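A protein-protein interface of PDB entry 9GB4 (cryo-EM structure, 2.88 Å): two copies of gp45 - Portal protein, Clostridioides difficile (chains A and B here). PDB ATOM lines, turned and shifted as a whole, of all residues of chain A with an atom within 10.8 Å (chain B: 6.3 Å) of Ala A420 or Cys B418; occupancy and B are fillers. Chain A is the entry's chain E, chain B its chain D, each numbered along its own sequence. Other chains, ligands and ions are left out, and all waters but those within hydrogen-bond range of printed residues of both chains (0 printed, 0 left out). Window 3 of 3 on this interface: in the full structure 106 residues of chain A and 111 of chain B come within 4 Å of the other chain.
The backbone NH (N) of Ala A420 sits close to the side-chain carboxylate (OE1) of Glu B415, at 3.4 Å.
The side-chain carboxylate of Glu B415 sits at hydrogen-bond distance from the side-chain sulfur of Cys A419 (3.5 Å).
The backbone carbonyl oxygen of Ala A420 lies within hydrogen-bond range of the side-chain sulfur of Cys B418 (3.7 Å).
Of the 23 printed residues of chain A, 5 touch a printed residue of chain B.
Printed residues of chain A that touch a printed residue of chain B: Lys A416, Cys A419, Ala A420, Lys A423 and Ala A424.
Hydrophobic or aromatic side chains of chain B within 4 Å of the printed part of chain A: Ala B411 and Leu B414.
Among the printed residues, no Asp or Glu carboxylate lies within 4 Å of a Lys or Arg side-chain nitrogen of the other chain.
Ala B411 touches Lys A416 (CB to CB, 3.4 Å).
CB of Ala A420 touches CG of Leu B414, at 3.9 Å.
CB of Lys A423 touches SG of Cys B418 (3.6 Å).
Ala A424 touches Cys B418.
N of Ala A424 touches OD2 of Asp B422, at 3.8 Å.
O of Glu B415 sits at hydrogen-bond distance from SG of Cys B419 (3.5 Å).
O of Lys A416 lies within hydrogen-bond range of SG of Cys A419 (3.1 Å).
O of Glu A415 is in hydrogen-bond range of SG of Cys A419 (3.3 Å).
Of chain B, only Leu B414, Glu B415 and Cys B418 come within 4 Å of Ala A420.
Of chain A, only Ala A420, Lys A423 and Ala A424 come within 4 Å of Cys B418.
Leu B414 touches one residue of chain A.
No residue of chain A comes within 4 Å of Val B417.
No residue of chain A comes within 4 Å of Cys B419.
No residue of chain A comes within 4 Å of Ala B420.
No residue of chain A comes within 4 Å of Leu B421.
Of the printed residues of chain B, Lys A423 touches Cys B418.
Of the printed residues of chain B, Lys A416 touches Ala B411.
Of the printed residues of chain B, Cys A419 touches Glu B415 (3.5 Å).
Val A417 touches none of the printed residues of chain B.
Ser A434 touches none of the printed residues of chain B.
The nearest printed residue of chain A that does not touch Asp B422 is Lys A423 (4.8 Å).
Cys A419 touches Glu B415, but with the chains exchanged Glu A415 does not touch Cys B419 (12.4 Å).
Ala A420 touches Leu B414, but with the chains exchanged Leu A414 does not touch Ala B420 (17.5 Å).
Ala A420 touches Glu B415, but with the chains exchanged Glu A415 does not touch Ala B420 (15.0 Å).
Ala A420 touches Cys B418, but with the chains exchanged Cys A418 does not touch Ala B420 (14.3 Å).
Of the 8 pairs that touch across the chains among the printed residues, none has its exchanged pair printed and touching as well.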
ATOM      1  N   ALA A 411      15.312 -21.864   8.793  1.00  0.00           N
ATOM      2  CA  ALA A 411      15.486 -22.106   7.365  1.00  0.00           C
ATOM      3  C   ALA A 411      14.728 -21.084   6.525  1.00  0.00           C
ATOM      4  O   ALA A 411      15.179 -20.719   5.431  1.00  0.00           O
ATOM      5  CB  ALA A 411      15.025 -23.517   7.023  1.00  0.00           C
ATOM      6  N   GLU A 412      13.573 -20.624   7.009  1.00  0.00           N
ATOM      7  CA  GLU A 412      12.839 -19.583   6.301  1.00  0.00           C
ATOM      8  C   GLU A 412      13.671 -18.314   6.196  1.00  0.00           C
ATOM      9  O   GLU A 412      13.850 -17.761   5.104  1.00  0.00           O
ATOM     10  CB  GLU A 412      11.516 -19.300   7.011  1.00  0.00           C
ATOM     11  CG  GLU A 412      10.426 -20.317   6.726  1.00  0.00           C
ATOM     12  CD  GLU A 412       9.215 -20.136   7.621  1.00  0.00           C
ATOM     13  OE1 GLU A 412       8.923 -18.983   8.000  1.00  0.00           O
ATOM     14  OE2 GLU A 412       8.556 -21.146   7.947  1.00  0.00           O
ATOM     15  N   THR A 413      14.206 -17.843   7.325  1.00  0.00           N
ATOM     16  CA  THR A 413      15.048 -16.650   7.264  1.00  0.00           C
ATOM     17  C   THR A 413      16.331 -16.917   6.482  1.00  0.00           C
ATOM     18  O   THR A 413      16.873 -15.999   5.857  1.00  0.00           O
ATOM     19  CB  THR A 413      15.362 -16.117   8.669  1.00  0.00           C
ATOM     20  OG1 THR A 413      16.198 -14.956   8.567  1.00  0.00           O
ATOM     21  CG2 THR A 413      16.055 -17.146   9.536  1.00  0.00           C
ATOM     22  N   LEU A 414      16.816 -18.162   6.481  1.00  0.00           N
ATOM     23  CA  LEU A 414      17.975 -18.503   5.661  1.00  0.00           C
ATOM     24  C   LEU A 414      17.683 -18.266   4.185  1.00  0.00           C
ATOM     25  O   LEU A 414      18.470 -17.625   3.479  1.00  0.00           O
ATOM     26  CB  LEU A 414      18.375 -19.962   5.897  1.00  0.00           C
ATOM     27  CG  LEU A 414      19.491 -20.577   5.039  1.00  0.00           C
ATOM     28  CD1 LEU A 414      20.830 -19.858   5.162  1.00  0.00           C
ATOM     29  CD2 LEU A 414      19.650 -22.046   5.396  1.00  0.00           C
ATOM     30  N   GLU A 415      16.555 -18.785   3.697  1.00  0.00           N
ATOM     31  CA  GLU A 415      16.228 -18.587   2.289  1.00  0.00           C
ATOM     32  C   GLU A 415      15.914 -17.126   1.990  1.00  0.00           C
ATOM     33  O   GLU A 415      16.211 -16.645   0.889  1.00  0.00           O
ATOM     34  CB  GLU A 415      15.069 -19.497   1.865  1.00  0.00           C
ATOM     35  CG  GLU A 415      13.735 -19.263   2.568  1.00  0.00           C
ATOM     36  CD  GLU A 415      12.556 -19.883   1.835  1.00  0.00           C
ATOM     37  OE1 GLU A 415      12.547 -19.877   0.587  1.00  0.00           O
ATOM     38  OE2 GLU A 415      11.629 -20.370   2.515  1.00  0.00           O
ATOM     39  N   LYS A 416      15.325 -16.402   2.948  1.00  0.00           N
ATOM     40  CA  LYS A 416      15.099 -14.974   2.739  1.00  0.00           C
ATOM     41  C   LYS A 416      16.420 -14.231   2.575  1.00  0.00           C
ATOM     42  O   LYS A 416      16.548 -13.366   1.701  1.00  0.00           O
ATOM     43  CB  LYS A 416      14.292 -14.370   3.895  1.00  0.00           C
ATOM     44  CG  LYS A 416      12.819 -14.809   4.043  1.00  0.00           C
ATOM     45  CD  LYS A 416      12.034 -14.956   2.733  1.00  0.00           C
ATOM     46  CE  LYS A 416      11.969 -13.657   1.938  1.00  0.00           C
ATOM     47  NZ  LYS A 416      11.344 -13.863   0.602  1.00  0.00           N
ATOM     48  N   VAL A 417      17.416 -14.558   3.400  1.00  0.00           N
ATOM     49  CA  VAL A 417      18.737 -13.951   3.249  1.00  0.00           C
ATOM     50  C   VAL A 417      19.343 -14.335   1.906  1.00  0.00           C
ATOM     51  O   VAL A 417      19.946 -13.504   1.216  1.00  0.00           O
ATOM     52  CB  VAL A 417      19.653 -14.361   4.417  1.00  0.00           C
ATOM     53  CG1 VAL A 417      21.109 -14.001   4.124  1.00  0.00           C
ATOM     54  CG2 VAL A 417      19.198 -13.697   5.692  1.00  0.00           C
ATOM     55  N   CYS A 418      19.208 -15.607   1.527  1.00  0.00           N
ATOM     56  CA  CYS A 418      19.833 -16.082   0.297  1.00  0.00           C
ATOM     57  C   CYS A 418      19.263 -15.373  -0.924  1.00  0.00           C
ATOM     58  O   CYS A 418      20.014 -14.953  -1.812  1.00  0.00           O
ATOM     59  CB  CYS A 418      19.654 -17.594   0.169  1.00  0.00           C
ATOM     60  SG  CYS A 418      20.602 -18.330  -1.179  1.00  0.00           S
ATOM     61  N   CYS A 419      17.941 -15.222  -0.987  1.00  0.00           N
ATOM     62  CA  CYS A 419      17.320 -14.520  -2.101  1.00  0.00           C
ATOM     63  C   CYS A 419      17.509 -13.012  -2.020  1.00  0.00           C
ATOM     64  O   CYS A 419      17.534 -12.352  -3.065  1.00  0.00           O
ATOM     65  CB  CYS A 419      15.823 -14.837  -2.171  1.00  0.00           C
ATOM     66  SG  CYS A 419      14.853 -14.131  -0.832  1.00  0.00           S
ATOM     67  N   ALA A 420      17.640 -12.453  -0.815  1.00  0.00           N
ATOM     68  CA  ALA A 420      17.949 -11.032  -0.690  1.00  0.00           C
ATOM     69  C   ALA A 420      19.303 -10.718  -1.308  1.00  0.00           C
ATOM     70  O   ALA A 420      19.455  -9.710  -2.007  1.00  0.00           O
ATOM     71  CB  ALA A 420      17.919 -10.615   0.778  1.00  0.00           C
ATOM     72  N   LEU A 421      20.293 -11.570  -1.065  1.00  0.00           N
ATOM     73  CA  LEU A 421      21.546 -11.490  -1.792  1.00  0.00           C
ATOM     74  C   LEU A 421      21.328 -11.982  -3.223  1.00  0.00           C
ATOM     75  O   LEU A 421      20.214 -12.331  -3.624  1.00  0.00           O
ATOM     76  CB  LEU A 421      22.626 -12.290  -1.068  1.00  0.00           C
ATOM     77  CG  LEU A 421      22.925 -11.840   0.367  1.00  0.00           C
ATOM     78  CD1 LEU A 421      23.864 -12.823   1.049  1.00  0.00           C
ATOM     79  CD2 LEU A 421      23.509 -10.432   0.395  1.00  0.00           C
ATOM     80  N   ASP A 422      22.401 -11.981  -4.010  1.00  0.00           N
ATOM     81  CA  ASP A 422      22.378 -12.242  -5.449  1.00  0.00           C
ATOM     82  C   ASP A 422      21.550 -11.212  -6.219  1.00  0.00           C
ATOM     83  O   ASP A 422      21.198 -11.448  -7.382  1.00  0.00           O
ATOM     84  CB  ASP A 422      21.870 -13.662  -5.762  1.00  0.00           C
ATOM     85  CG  ASP A 422      22.829 -14.742  -5.298  1.00  0.00           C
ATOM     86  OD1 ASP A 422      24.051 -14.487  -5.259  1.00  0.00           O
ATOM     87  OD2 ASP A 422      22.357 -15.850  -4.969  1.00  0.00           O
ATOM     88  N   LYS A 423      21.234 -10.074  -5.602  1.00  0.00           N
ATOM     89  CA  LYS A 423      20.517  -8.982  -6.238  1.00  0.00           C
ATOM     90  C   LYS A 423      21.054  -7.686  -5.653  1.00  0.00           C
ATOM     91  O   LYS A 423      21.598  -7.668  -4.545  1.00  0.00           O
ATOM     92  CB  LYS A 423      19.001  -9.090  -6.028  1.00  0.00           C
ATOM     93  CG  LYS A 423      18.361 -10.280  -6.728  1.00  0.00           C
ATOM     94  CD  LYS A 423      16.863 -10.332  -6.482  1.00  0.00           C
ATOM     95  CE  LYS A 423      16.251 -11.591  -7.073  1.00  0.00           C
ATOM     96  NZ  LYS A 423      14.789 -11.674  -6.811  1.00  0.00           N
ATOM     97  N   ALA A 424      20.893  -6.597  -6.401  1.00  0.00           N
ATOM     98  CA  ALA A 424      21.586  -5.346  -6.102  1.00  0.00           C
ATOM     99  C   ALA A 424      23.089  -5.613  -6.027  1.00  0.00           C
ATOM    100  O   ALA A 424      23.730  -5.489  -4.982  1.00  0.00           O
ATOM    101  CB  ALA A 424      21.062  -4.710  -4.812  1.00  0.00           C
ATOM    102  N   LEU A 425      23.642  -5.986  -7.183  1.00  0.00           N
ATOM    103  CA  LEU A 425      24.928  -6.671  -7.249  1.00  0.00           C
ATOM    104  C   LEU A 425      26.106  -5.811  -6.806  1.00  0.00           C
ATOM    105  O   LEU A 425      27.219  -6.337  -6.698  1.00  0.00           O
ATOM    106  CB  LEU A 425      25.160  -7.175  -8.677  1.00  0.00           C
ATOM    107  CG  LEU A 425      24.048  -8.046  -9.277  1.00  0.00           C
ATOM    108  CD1 LEU A 425      24.396  -8.447 -10.701  1.00  0.00           C
ATOM    109  CD2 LEU A 425      23.777  -9.281  -8.425  1.00  0.00           C
ATOM    110  N   GLU A 426      25.902  -4.517  -6.544  1.00  0.00           N
ATOM    111  CA  GLU A 426      26.973  -3.668  -6.032  1.00  0.00           C
ATOM    112  C   GLU A 426      27.228  -3.852  -4.537  1.00  0.00           C
ATOM    113  O   GLU A 426      27.973  -3.052  -3.962  1.00  0.00           O
ATOM    114  CB  GLU A 426      26.650  -2.199  -6.317  1.00  0.00           C
ATOM    115  CG  GLU A 426      26.395  -1.874  -7.789  1.00  0.00           C
ATOM    116  CD  GLU A 426      27.566  -2.226  -8.686  1.00  0.00           C
ATOM    117  OE1 GLU A 426      28.720  -2.160  -8.213  1.00  0.00           O
ATOM    118  OE2 GLU A 426      27.333  -2.568  -9.865  1.00  0.00           O
ATOM    119  N   GLY A 427      26.641  -4.865  -3.892  1.00  0.00           N
ATOM    120  CA  GLY A 427      26.885  -5.098  -2.479  1.00  0.00           C
ATOM    121  C   GLY A 427      28.324  -5.432  -2.147  1.00  0.00           C
ATOM    122  O   GLY A 427      28.812  -5.036  -1.082  1.00  0.00           O
ATOM    123  N   GLY A 428      29.015  -6.156  -3.029  1.00  0.00           N
ATOM    124  CA  GLY A 428      30.419  -6.470  -2.836  1.00  0.00           C
ATOM    125  C   GLY A 428      30.661  -7.888  -2.337  1.00  0.00           C
ATOM    126  O   GLY A 428      29.836  -8.793  -2.474  1.00  0.00           O
ATOM    127  N   SER A 431      28.923 -10.176   1.082  1.00  0.00           N
ATOM    128  CA  SER A 431      27.768 -11.067   1.035  1.00  0.00           C
ATOM    129  C   SER A 431      28.165 -12.499   1.376  1.00  0.00           C
ATOM    130  O   SER A 431      27.475 -13.185   2.140  1.00  0.00           O
ATOM    131  CB  SER A 431      27.119 -11.005  -0.348  1.00  0.00           C
ATOM    132  OG  SER A 431      28.075 -11.225  -1.370  1.00  0.00           O
ATOM    133  N   GLU A 432      29.280 -12.970   0.811  1.00  0.00           N
ATOM    134  CA  GLU A 432      29.759 -14.308   1.136  1.00  0.00           C
ATOM    135  C   GLU A 432      30.165 -14.402   2.601  1.00  0.00           C
ATOM    136  O   GLU A 432      29.895 -15.411   3.262  1.00  0.00           O
ATOM    137  CB  GLU A 432      30.930 -14.679   0.222  1.00  0.00           C
ATOM    138  CG  GLU A 432      31.478 -16.095   0.406  1.00  0.00           C
ATOM    139  CD  GLU A 432      30.436 -17.171   0.161  1.00  0.00           C
ATOM    140  OE1 GLU A 432      29.442 -16.892  -0.542  1.00  0.00           O
ATOM    141  OE2 GLU A 432      30.609 -18.298   0.673  1.00  0.00           O
ATOM    142  N   SER A 434      28.883 -12.771   5.067  1.00  0.00           N
ATOM    143  CA  SER A 434      27.663 -12.842   5.859  1.00  0.00           C
ATOM    144  C   SER A 434      27.009 -14.215   5.754  1.00  0.00           C
ATOM    145  O   SER A 434      26.608 -14.800   6.767  1.00  0.00           O
ATOM    146  CB  SER A 434      26.686 -11.754   5.413  1.00  0.00           C
ATOM    147  OG  SER A 434      25.416 -11.933   6.017  1.00  0.00           O
ATOM    148  N   THR A 435      26.894 -14.751   4.536  1.00  0.00           N
ATOM    149  CA  THR A 435      26.120 -15.975   4.365  1.00  0.00           C
ATOM    150  C   THR A 435      26.866 -17.188   4.916  1.00  0.00           C
ATOM    151  O   THR A 435      26.240 -18.103   5.461  1.00  0.00           O
ATOM    152  CB  THR A 435      25.746 -16.177   2.892  1.00  0.00           C
ATOM    153  OG1 THR A 435      24.708 -17.159   2.791  1.00  0.00           O
ATOM    154  CG2 THR A 435      26.935 -16.636   2.068  1.00  0.00           C
ATOM    155  N   PHE A 438      26.241 -17.124   8.503  1.00  0.00           N
ATOM    156  CA  PHE A 438      24.873 -17.541   8.788  1.00  0.00           C
ATOM    157  C   PHE A 438      24.748 -19.056   8.723  1.00  0.00           C
ATOM    158  O   PHE A 438      24.065 -19.666   9.549  1.00  0.00           O
ATOM    159  CB  PHE A 438      23.893 -16.889   7.812  1.00  0.00           C
ATOM    160  CG  PHE A 438      22.455 -17.038   8.224  1.00  0.00           C
ATOM    161  CD1 PHE A 438      21.833 -16.048   8.954  1.00  0.00           C
ATOM    162  CD2 PHE A 438      21.739 -18.179   7.916  1.00  0.00           C
ATOM    163  CE1 PHE A 438      20.522 -16.180   9.352  1.00  0.00           C
ATOM    164  CE2 PHE A 438      20.432 -18.316   8.314  1.00  0.00           C
ATOM    165  CZ  PHE A 438      19.822 -17.316   9.031  1.00  0.00           C
ATOM    166  N   ALA B 411      14.831  -9.956   7.477  1.00  0.00           N
ATOM    167  CA  ALA B 411      15.064 -10.437   6.120  1.00  0.00           C
ATOM    168  C   ALA B 411      13.952 -10.005   5.176  1.00  0.00           C
ATOM    169  O   ALA B 411      14.218  -9.677   4.016  1.00  0.00           O
ATOM    170  CB  ALA B 411      15.189 -11.957   6.118  1.00  0.00           C
ATOM    171  N   THR B 413      12.024  -7.262   5.370  1.00  0.00           N
ATOM    172  CA  THR B 413      12.177  -5.852   5.015  1.00  0.00           C
ATOM    173  C   THR B 413      13.403  -5.638   4.133  1.00  0.00           C
ATOM    174  O   THR B 413      13.400  -4.759   3.265  1.00  0.00           O
ATOM    175  CB  THR B 413      12.236  -4.960   6.263  1.00  0.00           C
ATOM    176  OG1 THR B 413      12.429  -3.597   5.865  1.00  0.00           O
ATOM    177  CG2 THR B 413      13.354  -5.354   7.199  1.00  0.00           C
ATOM    178  N   LEU B 414      14.457  -6.436   4.327  1.00  0.00           N
ATOM    179  CA  LEU B 414      15.608  -6.350   3.430  1.00  0.00           C
ATOM    180  C   LEU B 414      15.219  -6.731   2.007  1.00  0.00           C
ATOM    181  O   LEU B 414      15.639  -6.081   1.044  1.00  0.00           O
ATOM    182  CB  LEU B 414      16.739  -7.244   3.938  1.00  0.00           C
ATOM    183  CG  LEU B 414      17.964  -7.417   3.033  1.00  0.00           C
ATOM    184  CD1 LEU B 414      18.547  -6.081   2.590  1.00  0.00           C
ATOM    185  CD2 LEU B 414      19.019  -8.241   3.748  1.00  0.00           C
ATOM    186  N   GLU B 415      14.421  -7.788   1.858  1.00  0.00           N
ATOM    187  CA  GLU B 415      13.938  -8.187   0.541  1.00  0.00           C
ATOM    188  C   GLU B 415      13.088  -7.085  -0.077  1.00  0.00           C
ATOM    189  O   GLU B 415      13.180  -6.806  -1.280  1.00  0.00           O
ATOM    190  CB  GLU B 415      13.140  -9.490   0.660  1.00  0.00           C
ATOM    191  CG  GLU B 415      12.570 -10.036  -0.649  1.00  0.00           C
ATOM    192  CD  GLU B 415      13.643 -10.392  -1.655  1.00  0.00           C
ATOM    193  OE1 GLU B 415      14.784 -10.675  -1.234  1.00  0.00           O
ATOM    194  OE2 GLU B 415      13.346 -10.394  -2.869  1.00  0.00           O
ATOM    195  N   LYS B 416      12.240  -6.455   0.739  1.00  0.00           N
ATOM    196  CA  LYS B 416      11.408  -5.367   0.238  1.00  0.00           C
ATOM    197  C   LYS B 416      12.261  -4.200  -0.243  1.00  0.00           C
ATOM    198  O   LYS B 416      11.989  -3.613  -1.297  1.00  0.00           O
ATOM    199  CB  LYS B 416      10.435  -4.909   1.324  1.00  0.00           C
ATOM    200  CG  LYS B 416       9.308  -5.889   1.612  1.00  0.00           C
ATOM    201  CD  LYS B 416       8.233  -5.839   0.539  1.00  0.00           C
ATOM    202  CE  LYS B 416       7.067  -6.752   0.879  1.00  0.00           C
ATOM    203  NZ  LYS B 416       7.388  -8.185   0.636  1.00  0.00           N
ATOM    204  N   VAL B 417      13.305  -3.854   0.512  1.00  0.00           N
ATOM    205  CA  VAL B 417      14.210  -2.786   0.094  1.00  0.00           C
ATOM    206  C   VAL B 417      14.903  -3.163  -1.208  1.00  0.00           C
ATOM    207  O   VAL B 417      15.026  -2.345  -2.127  1.00  0.00           O
ATOM    208  CB  VAL B 417      15.233  -2.484   1.204  1.00  0.00           C
ATOM    209  CG1 VAL B 417      16.360  -1.597   0.683  1.00  0.00           C
ATOM    210  CG2 VAL B 417      14.557  -1.823   2.380  1.00  0.00           C
ATOM    211  N   CYS B 418      15.379  -4.406  -1.300  1.00  0.00           N
ATOM    212  CA  CYS B 418      16.129  -4.825  -2.478  1.00  0.00           C
ATOM    213  C   CYS B 418      15.260  -4.793  -3.726  1.00  0.00           C
ATOM    214  O   CYS B 418      15.698  -4.324  -4.783  1.00  0.00           O
ATOM    215  CB  CYS B 418      16.705  -6.223  -2.263  1.00  0.00           C
ATOM    216  SG  CYS B 418      17.908  -6.715  -3.517  1.00  0.00           S
ATOM    217  N   CYS B 419      14.025  -5.282  -3.630  1.00  0.00           N
ATOM    218  CA  CYS B 419      13.128  -5.247  -4.776  1.00  0.00           C
ATOM    219  C   CYS B 419      12.656  -3.838  -5.100  1.00  0.00           C
ATOM    220  O   CYS B 419      12.432  -3.531  -6.276  1.00  0.00           O
ATOM    221  CB  CYS B 419      11.911  -6.147  -4.544  1.00  0.00           C
ATOM    222  SG  CYS B 419      10.714  -5.514  -3.357  1.00  0.00           S
ATOM    223  N   ALA B 420      12.497  -2.978  -4.089  1.00  0.00           N
ATOM    224  CA  ALA B 420      12.156  -1.586  -4.357  1.00  0.00           C
ATOM    225  C   ALA B 420      13.256  -0.899  -5.152  1.00  0.00           C
ATOM    226  O   ALA B 420      12.977  -0.181  -6.119  1.00  0.00           O
ATOM    227  CB  ALA B 420      11.901  -0.845  -3.046  1.00  0.00           C
ATOM    228  N   LEU B 421      14.511  -1.112  -4.769  1.00  0.00           N
ATOM    229  CA  LEU B 421      15.619  -0.606  -5.559  1.00  0.00           C
ATOM    230  C   LEU B 421      15.712  -1.378  -6.874  1.00  0.00           C
ATOM    231  O   LEU B 421      14.963  -2.326  -7.125  1.00  0.00           O
ATOM    232  CB  LEU B 421      16.924  -0.704  -4.768  1.00  0.00           C
ATOM    233  CG  LEU B 421      16.956   0.067  -3.443  1.00  0.00           C
ATOM    234  CD1 LEU B 421      18.233  -0.244  -2.677  1.00  0.00           C
ATOM    235  CD2 LEU B 421      16.822   1.567  -3.673  1.00  0.00           C
ATOM    236  N   ASP B 422      16.639  -0.943  -7.728  1.00  0.00           N
ATOM    237  CA  ASP B 422      16.759  -1.407  -9.112  1.00  0.00           C
ATOM    238  C   ASP B 422      15.548  -1.018  -9.960  1.00  0.00           C
ATOM    239  O   ASP B 422      15.345  -1.568 -11.047  1.00  0.00           O
ATOM    240  CB  ASP B 422      16.980  -2.924  -9.183  1.00  0.00           C
ATOM    241  CG  ASP B 422      18.066  -3.400  -8.238  1.00  0.00           C
ATOM    242  OD1 ASP B 422      18.905  -2.572  -7.829  1.00  0.00           O
ATOM    243  OD2 ASP B 422      18.077  -4.603  -7.904  1.00  0.00           O
ATOM    244  N   THR B 435      21.678   0.205   0.860  1.00  0.00           N
ATOM    245  CA  THR B 435      21.597  -1.249   0.943  1.00  0.00           C
ATOM    246  C   THR B 435      22.810  -1.835   1.662  1.00  0.00           C
ATOM    247  O   THR B 435      22.670  -2.792   2.431  1.00  0.00           O
ATOM    248  CB  THR B 435      21.413  -1.862  -0.453  1.00  0.00           C
ATOM    249  OG1 THR B 435      20.905  -3.196  -0.323  1.00  0.00           O
ATOM    250  CG2 THR B 435      22.711  -1.906  -1.245  1.00  0.00           C
